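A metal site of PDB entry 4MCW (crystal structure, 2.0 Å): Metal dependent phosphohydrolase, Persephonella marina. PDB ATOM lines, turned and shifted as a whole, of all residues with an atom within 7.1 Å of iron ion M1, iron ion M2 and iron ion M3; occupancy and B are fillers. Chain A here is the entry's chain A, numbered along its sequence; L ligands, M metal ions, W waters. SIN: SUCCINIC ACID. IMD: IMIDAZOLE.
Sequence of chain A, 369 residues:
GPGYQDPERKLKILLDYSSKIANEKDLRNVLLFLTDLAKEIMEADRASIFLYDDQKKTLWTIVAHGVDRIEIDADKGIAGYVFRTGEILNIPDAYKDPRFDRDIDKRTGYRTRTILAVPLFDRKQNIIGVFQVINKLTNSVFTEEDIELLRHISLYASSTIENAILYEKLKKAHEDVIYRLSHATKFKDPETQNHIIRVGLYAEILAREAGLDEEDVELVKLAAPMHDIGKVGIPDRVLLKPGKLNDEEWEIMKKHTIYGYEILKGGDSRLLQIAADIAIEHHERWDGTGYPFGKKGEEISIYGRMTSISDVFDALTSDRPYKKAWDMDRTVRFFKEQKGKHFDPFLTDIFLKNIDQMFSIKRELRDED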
ATOM      1  N   ASP A 189      15.161  14.089 -32.088  1.00  0.00           N
ATOM      2  CA  ASP A 189      14.515  12.795 -31.816  1.00  0.00           C
ATOM      3  C   ASP A 189      14.403  12.063 -33.138  1.00  0.00           C
ATOM      4  O   ASP A 189      14.177  12.689 -34.155  1.00  0.00           O
ATOM      5  CB  ASP A 189      13.157  12.987 -31.158  1.00  0.00           C
ATOM      6  CG  ASP A 189      12.451  11.675 -30.838  1.00  0.00           C
ATOM      7  OD1 ASP A 189      11.783  11.140 -31.740  1.00  0.00           O
ATOM      8  OD2 ASP A 189      12.551  11.187 -29.681  1.00  0.00           O
ATOM      9  N   GLU A 191      12.107   9.756 -34.304  1.00  0.00           N
ATOM     10  CA  GLU A 191      10.768   9.403 -34.883  1.00  0.00           C
ATOM     11  C   GLU A 191      10.565  10.167 -36.202  1.00  0.00           C
ATOM     12  O   GLU A 191      10.748  11.414 -36.245  1.00  0.00           O
ATOM     13  CB  GLU A 191       9.623   9.604 -33.886  1.00  0.00           C
ATOM     14  CG  GLU A 191       9.723   8.706 -32.643  1.00  0.00           C
ATOM     15  CD  GLU A 191       8.428   8.457 -31.886  1.00  0.00           C
ATOM     16  OE1 GLU A 191       8.456   8.264 -30.631  1.00  0.00           O
ATOM     17  OE2 GLU A 191       7.346   8.442 -32.524  1.00  0.00           O
ATOM     18  N   HIS A 195       6.298   8.014 -39.979  1.00  0.00           N
ATOM     19  CA  HIS A 195       5.788   7.331 -38.801  1.00  0.00           C
ATOM     20  C   HIS A 195       4.663   8.102 -38.190  1.00  0.00           C
ATOM     21  O   HIS A 195       3.622   7.538 -37.816  1.00  0.00           O
ATOM     22  CB  HIS A 195       6.922   7.120 -37.818  1.00  0.00           C
ATOM     23  CG  HIS A 195       6.458   6.788 -36.437  1.00  0.00           C
ATOM     24  ND1 HIS A 195       5.975   5.560 -36.106  1.00  0.00           N
ATOM     25  CD2 HIS A 195       6.449   7.544 -35.277  1.00  0.00           C
ATOM     26  CE1 HIS A 195       5.653   5.549 -34.795  1.00  0.00           C
ATOM     27  NE2 HIS A 195       5.990   6.754 -34.278  1.00  0.00           N
ATOM     28  N   ILE A 196       4.893   9.404 -38.005  1.00  0.00           N
ATOM     29  CA  ILE A 196       3.896  10.312 -37.440  1.00  0.00           C
ATOM     30  C   ILE A 196       2.590  10.294 -38.266  1.00  0.00           C
ATOM     31  O   ILE A 196       1.528  10.253 -37.696  1.00  0.00           O
ATOM     32  CB  ILE A 196       4.504  11.748 -37.355  1.00  0.00           C
ATOM     33  CG1 ILE A 196       5.492  11.819 -36.188  1.00  0.00           C
ATOM     34  CG2 ILE A 196       3.443  12.831 -37.301  1.00  0.00           C
ATOM     35  CD1 ILE A 196       6.514  12.947 -36.360  1.00  0.00           C
ATOM     36  N   VAL A 199       0.794   6.553 -38.053  1.00  0.00           N
ATOM     37  CA  VAL A 199       0.128   6.202 -36.787  1.00  0.00           C
ATOM     38  C   VAL A 199      -1.316   6.749 -36.725  1.00  0.00           C
ATOM     39  O   VAL A 199      -2.223   6.061 -36.231  1.00  0.00           O
ATOM     40  CB  VAL A 199       0.959   6.626 -35.564  1.00  0.00           C
ATOM     41  CG1 VAL A 199       0.188   6.470 -34.274  1.00  0.00           C
ATOM     42  CG2 VAL A 199       2.220   5.752 -35.456  1.00  0.00           C
ATOM     43  N   HIS A 227       1.009  13.141 -30.496  1.00  0.00           N
ATOM     44  CA  HIS A 227       1.047  12.639 -29.137  1.00  0.00           C
ATOM     45  C   HIS A 227       2.417  12.792 -28.484  1.00  0.00           C
ATOM     46  O   HIS A 227       2.496  12.761 -27.283  1.00  0.00           O
ATOM     47  CB  HIS A 227       0.561  11.181 -29.027  1.00  0.00           C
ATOM     48  CG  HIS A 227       1.467  10.175 -29.691  1.00  0.00           C
ATOM     49  ND1 HIS A 227       1.311   9.802 -30.981  1.00  0.00           N
ATOM     50  CD2 HIS A 227       2.599   9.502 -29.226  1.00  0.00           C
ATOM     51  CE1 HIS A 227       2.276   8.904 -31.306  1.00  0.00           C
ATOM     52  NE2 HIS A 227       3.064   8.724 -30.230  1.00  0.00           N
ATOM     53  N   ASP A 228       3.482  12.962 -29.255  1.00  0.00           N
ATOM     54  CA  ASP A 228       4.827  13.060 -28.654  1.00  0.00           C
ATOM     55  C   ASP A 228       5.389  14.476 -28.648  1.00  0.00           C
ATOM     56  O   ASP A 228       6.606  14.658 -28.423  1.00  0.00           O
ATOM     57  CB  ASP A 228       5.833  12.196 -29.430  1.00  0.00           C
ATOM     58  CG  ASP A 228       6.035  10.820 -28.837  1.00  0.00           C
ATOM     59  OD1 ASP A 228       5.673  10.488 -27.687  1.00  0.00           O
ATOM     60  OD2 ASP A 228       6.641  10.044 -29.558  1.00  0.00           O
ATOM     61  N   LYS A 231       7.953  16.105 -26.154  1.00  0.00           N
ATOM     62  CA  LYS A 231       9.399  15.868 -26.173  1.00  0.00           C
ATOM     63  C   LYS A 231      10.178  17.197 -26.314  1.00  0.00           C
ATOM     64  O   LYS A 231      11.338  17.279 -25.896  1.00  0.00           O
ATOM     65  CB  LYS A 231       9.782  14.909 -27.294  1.00  0.00           C
ATOM     66  CG  LYS A 231       9.402  13.470 -26.969  1.00  0.00           C
ATOM     67  CD  LYS A 231       9.940  12.549 -28.039  1.00  0.00           C
ATOM     68  CE  LYS A 231       9.546  11.094 -27.755  1.00  0.00           C
ATOM     69  NZ  LYS A 231       9.738  10.285 -28.996  1.00  0.00           N
ATOM     70  N   MET A 253      12.087  11.827 -18.699  1.00  0.00           N
ATOM     71  CA  MET A 253      11.657  11.437 -20.036  1.00  0.00           C
ATOM     72  C   MET A 253      10.153  11.124 -20.066  1.00  0.00           C
ATOM     73  O   MET A 253       9.460  11.477 -21.009  1.00  0.00           O
ATOM     74  CB  MET A 253      12.452  10.231 -20.557  1.00  0.00           C
ATOM     75  CG  MET A 253      12.146   9.908 -21.996  1.00  0.00           C
ATOM     76  SD  MET A 253      12.751  11.201 -23.102  1.00  0.00           S
ATOM     77  CE  MET A 253      11.547  11.093 -24.426  1.00  0.00           C
ATOM     78  N   HIS A 256       7.234  13.678 -20.832  1.00  0.00           N
ATOM     79  CA  HIS A 256       6.869  14.183 -22.171  1.00  0.00           C
ATOM     80  C   HIS A 256       5.381  14.013 -22.393  1.00  0.00           C
ATOM     81  O   HIS A 256       4.800  14.703 -23.229  1.00  0.00           O
ATOM     82  CB  HIS A 256       7.661  13.545 -23.287  1.00  0.00           C
ATOM     83  CG  HIS A 256       7.170  12.149 -23.688  1.00  0.00           C
ATOM     84  ND1 HIS A 256       7.397  11.056 -22.934  1.00  0.00           N
ATOM     85  CD2 HIS A 256       6.443  11.720 -24.800  1.00  0.00           C
ATOM     86  CE1 HIS A 256       6.854   9.984 -23.524  1.00  0.00           C
ATOM     87  NE2 HIS A 256       6.262  10.394 -24.668  1.00  0.00           N
ATOM     88  N   THR A 257       4.754  13.126 -21.615  1.00  0.00           N
ATOM     89  CA  THR A 257       3.316  12.920 -21.677  1.00  0.00           C
ATOM     90  C   THR A 257       2.563  14.142 -21.103  1.00  0.00           C
ATOM     91  O   THR A 257       1.670  14.703 -21.764  1.00  0.00           O
ATOM     92  CB  THR A 257       2.907  11.634 -20.924  1.00  0.00           C
ATOM     93  OG1 THR A 257       3.358  11.721 -19.563  1.00  0.00           O
ATOM     94  CG2 THR A 257       3.536  10.391 -21.612  1.00  0.00           C
ATOM     95  N   ALA A 279      -1.853  12.631 -25.872  1.00  0.00           N
ATOM     96  CA  ALA A 279      -0.505  12.992 -25.453  1.00  0.00           C
ATOM     97  C   ALA A 279      -0.270  12.494 -24.039  1.00  0.00           C
ATOM     98  O   ALA A 279       0.766  11.895 -23.750  1.00  0.00           O
ATOM     99  CB  ALA A 279      -0.246  14.506 -25.568  1.00  0.00           C
ATOM    100  N   HIS A 282      -0.926   7.938 -23.928  1.00  0.00           N
ATOM    101  CA  HIS A 282      -0.457   6.947 -24.862  1.00  0.00           C
ATOM    102  C   HIS A 282       0.533   5.922 -24.299  1.00  0.00           C
ATOM    103  O   HIS A 282       0.780   4.932 -24.956  1.00  0.00           O
ATOM    104  CB  HIS A 282       0.007   7.560 -26.170  1.00  0.00           C
ATOM    105  CG  HIS A 282       1.295   8.333 -26.062  1.00  0.00           C
ATOM    106  ND1 HIS A 282       1.341   9.608 -25.578  1.00  0.00           N
ATOM    107  CD2 HIS A 282       2.597   7.981 -26.382  1.00  0.00           C
ATOM    108  CE1 HIS A 282       2.621  10.039 -25.588  1.00  0.00           C
ATOM    109  NE2 HIS A 282       3.389   9.058 -26.078  1.00  0.00           N
ATOM    110  N   HIS A 283       1.076   6.153 -23.088  1.00  0.00           N
ATOM    111  CA  HIS A 283       1.953   5.159 -22.438  1.00  0.00           C
ATOM    112  C   HIS A 283       1.236   4.483 -21.307  1.00  0.00           C
ATOM    113  O   HIS A 283       1.830   3.712 -20.587  1.00  0.00           O
ATOM    114  CB  HIS A 283       3.302   5.778 -21.939  1.00  0.00           C
ATOM    115  CG  HIS A 283       4.188   6.276 -23.065  1.00  0.00           C
ATOM    116  ND1 HIS A 283       4.951   5.448 -23.800  1.00  0.00           N
ATOM    117  CD2 HIS A 283       4.399   7.565 -23.575  1.00  0.00           C
ATOM    118  CE1 HIS A 283       5.613   6.181 -24.761  1.00  0.00           C
ATOM    119  NE2 HIS A 283       5.270   7.482 -24.600  1.00  0.00           N
ATOM    120  N   TYR A 291       2.465   4.404 -17.660  1.00  0.00           N
ATOM    121  CA  TYR A 291       2.735   5.715 -17.070  1.00  0.00           C
ATOM    122  C   TYR A 291       2.053   6.840 -17.856  1.00  0.00           C
ATOM    123  O   TYR A 291       1.696   6.645 -19.036  1.00  0.00           O
ATOM    124  CB  TYR A 291       4.247   5.951 -16.960  1.00  0.00           C
ATOM    125  CG  TYR A 291       5.017   5.924 -18.287  1.00  0.00           C
ATOM    126  CD1 TYR A 291       5.529   4.727 -18.778  1.00  0.00           C
ATOM    127  CD2 TYR A 291       5.253   7.091 -19.012  1.00  0.00           C
ATOM    128  CE1 TYR A 291       6.253   4.695 -19.960  1.00  0.00           C
ATOM    129  CE2 TYR A 291       5.984   7.070 -20.202  1.00  0.00           C
ATOM    130  CZ  TYR A 291       6.469   5.862 -20.662  1.00  0.00           C
ATOM    131  OH  TYR A 291       7.196   5.786 -21.839  1.00  0.00           O
ATOM    132  N   ASP A 311       0.827   2.862 -32.584  1.00  0.00           N
ATOM    133  CA  ASP A 311       2.220   3.297 -32.410  1.00  0.00           C
ATOM    134  C   ASP A 311       3.139   2.070 -32.217  1.00  0.00           C
ATOM    135  O   ASP A 311       4.157   1.968 -32.848  1.00  0.00           O
ATOM    136  CB  ASP A 311       2.280   4.186 -31.178  1.00  0.00           C
ATOM    137  CG  ASP A 311       3.578   4.977 -31.108  1.00  0.00           C
ATOM    138  OD1 ASP A 311       4.014   5.592 -32.109  1.00  0.00           O
ATOM    139  OD2 ASP A 311       4.183   4.968 -30.035  1.00  0.00           O
ATOM    140  N   VAL A 312       2.770   1.157 -31.338  1.00  0.00           N
ATOM    141  CA  VAL A 312       3.525  -0.129 -31.193  1.00  0.00           C
ATOM    142  C   VAL A 312       3.577  -0.908 -32.514  1.00  0.00           C
ATOM    143  O   VAL A 312       4.640  -1.425 -32.885  1.00  0.00           O
ATOM    144  CB  VAL A 312       2.965  -0.972 -30.047  1.00  0.00           C
ATOM    145  CG1 VAL A 312       3.687  -2.332 -29.949  1.00  0.00           C
ATOM    146  CG2 VAL A 312       3.109  -0.226 -28.732  1.00  0.00           C
ATOM    147  N   ASP A 314       3.485   0.216 -35.543  1.00  0.00           N
ATOM    148  CA  ASP A 314       4.415   0.843 -36.476  1.00  0.00           C
ATOM    149  C   ASP A 314       5.854   0.540 -36.077  1.00  0.00           C
ATOM    150  O   ASP A 314       6.697   0.305 -36.948  1.00  0.00           O
ATOM    151  CB  ASP A 314       4.223   2.390 -36.633  1.00  0.00           C
ATOM    152  CG  ASP A 314       4.761   2.879 -37.958  1.00  0.00           C
ATOM    153  OD1 ASP A 314       4.404   2.294 -39.004  1.00  0.00           O
ATOM    154  OD2 ASP A 314       5.570   3.820 -38.008  1.00  0.00           O
ATOM    155  N   ALA A 315       6.129   0.514 -34.788  1.00  0.00           N
ATOM    156  CA  ALA A 315       7.504   0.272 -34.309  1.00  0.00           C
ATOM    157  C   ALA A 315       7.934  -1.188 -34.531  1.00  0.00           C
ATOM    158  O   ALA A 315       9.048  -1.416 -34.950  1.00  0.00           O
ATOM    159  CB  ALA A 315       7.636   0.648 -32.841  1.00  0.00           C
HETATM  160  C1  SIN L   1       7.685   1.376 -29.341  1.00  0.00           C
HETATM  161  O1  SIN L   1       6.991   0.484 -28.837  1.00  0.00           O
HETATM  162  O2  SIN L   1       8.877   1.167 -29.678  1.00  0.00           O
HETATM  163  C2  SIN L   1       7.063   2.768 -29.545  1.00  0.00           C
HETATM  164  C3  SIN L   1       7.988   3.660 -30.378  1.00  0.00           C
HETATM  165  C4  SIN L   1       7.495   5.114 -30.471  1.00  0.00           C
HETATM  166  O3  SIN L   1       7.230   5.628 -31.588  1.00  0.00           O
HETATM  167  O4  SIN L   1       7.442   5.762 -29.423  1.00  0.00           O
HETATM  168  N1  IMD L   2       4.642   8.832 -32.933  1.00  0.00           N
HETATM  169  C2  IMD L   2       4.824  10.051 -32.385  1.00  0.00           C
HETATM  170  N3  IMD L   2       3.854  10.855 -32.870  1.00  0.00           N
HETATM  171  C4  IMD L   2       3.070  10.159 -33.724  1.00  0.00           C
HETATM  172  C5  IMD L   2       3.576   8.866 -33.767  1.00  0.00           C
HETATM  173  C1  SIN L   3       9.185   6.870 -23.770  1.00  0.00           C
HETATM  174  O1  SIN L   3       8.659   7.256 -22.682  1.00  0.00           O
HETATM  175  O2  SIN L   3       9.023   5.704 -24.259  1.00  0.00           O
HETATM  176  C2  SIN L   3      10.033   7.899 -24.474  1.00  0.00           C
HETATM  177  C3  SIN L   3      10.119   7.742 -25.992  1.00  0.00           C
HETATM  178  C4  SIN L   3       8.802   8.133 -26.645  1.00  0.00           C
HETATM  179  O3  SIN L   3       8.731   8.141 -27.889  1.00  0.00           O
HETATM  180  O4  SIN L   3       7.830   8.435 -25.932  1.00  0.00           O
HETATM  181 FE    FE M   1       5.706   7.064 -32.276  1.00  0.00          FE
HETATM  182 FE    FE M   2       7.069   7.952 -29.262  1.00  0.00          FE
HETATM  183 FE    FE M   3       5.530   8.945 -26.057  1.00  0.00          FE
HETATM  184  O   HOH W   1       6.014   7.835 -27.850  1.00  0.00           O
HETATM  185  O   HOH W   2       5.173   7.286 -30.485  1.00  0.00           O
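The side-chain carboxylate of Glu 191 lies close to the side-chain amino group of Lys 231 (2.9 Å).
N of Glu 191 is in hydrogen-bond range of OD1 of Asp 189.
The side-chain carboxylate of Asp 314 sits at hydrogen-bond distance from a ring nitrogen (ND1) of His 195.
OH of Tyr 291 lies within hydrogen-bond range of ND1 of His 283, 3.0 Å away.
The backbone carbonyl oxygen (O) of Met 253 lies within hydrogen-bond range of a ring nitrogen (ND1) of His 256 (2.9 Å).
A ring nitrogen (ND1) of His 282 sits at hydrogen-bond distance from the backbone carbonyl oxygen (O) of Ala 279 (3.0 Å).
NZ of Lys 231 sits close to OD2 of Asp 228, 3.2 Å away.
The side-chain amino group of Lys 231 is in salt-bridge range of the side-chain carboxylate of Asp 189.
Residues that only touch iron ion M1: His 227 (3.7 Å).
Along chain A the residues within 4 Å of iron ion M1 span positions 191 to 311.
The nearest printed residue that does not touch iron ion M1 is Asp 228 (4.1 Å).
Lys 231 touches iron ion M2 (NZ to FE, 3.6 Å).
Of the 19 residues printed, 3 come within 4 Å of iron ion M2.
Four residues have an atom within 4 Å of iron ion M3: Asp 228, His 256, His 282 and His 283.
Water W2 is bound to iron ion M1.
A ring nitrogen (NE2) of His 195 binds iron ion M1 (2.0 Å).
Iron ion M1 is bound by OE2 of Glu 191, 2.2 Å away.
N1 of IMD L2 is bound to iron ion M1, at 2.2 Å.
O3 of SIN L1 is bound to iron ion M1 (2.2 Å).
OD1 of Asp 311 binds iron ion M1.
Water W1 binds iron ion M2, 1.8 Å away.
The side-chain carboxylate (OE1) of Glu 191 binds iron ion M2 (2.0 Å).
Iron ion M2 is bound by OD2 of Asp 228, 2.2 Å away.
O3 of SIN L3 is bound to iron ion M2 (2.2 Å).
O4 of SIN L1 binds iron ion M2, 2.2 Å away.
Water W2 is bound to iron ion M2.
Iron ion M2 has six donor atoms within binding distance.
Iron ion M3 is bound by a ring nitrogen (NE2) of His 283 (2.1 Å).
A ring nitrogen (NE2) of His 256 binds iron ion M3 (2.1 Å).
NE2 of His 282 binds iron ion M3 (2.1 Å).
Water W1 binds iron ion M3.
OD1 of Asp 228 is bound to iron ion M3.
Iron ion M3 is bound by an oxygen (O4) of SIN L3.
Water W2 lies within hydrogen-bond range of OD2 of Asp 311 and NE2 of His 227.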
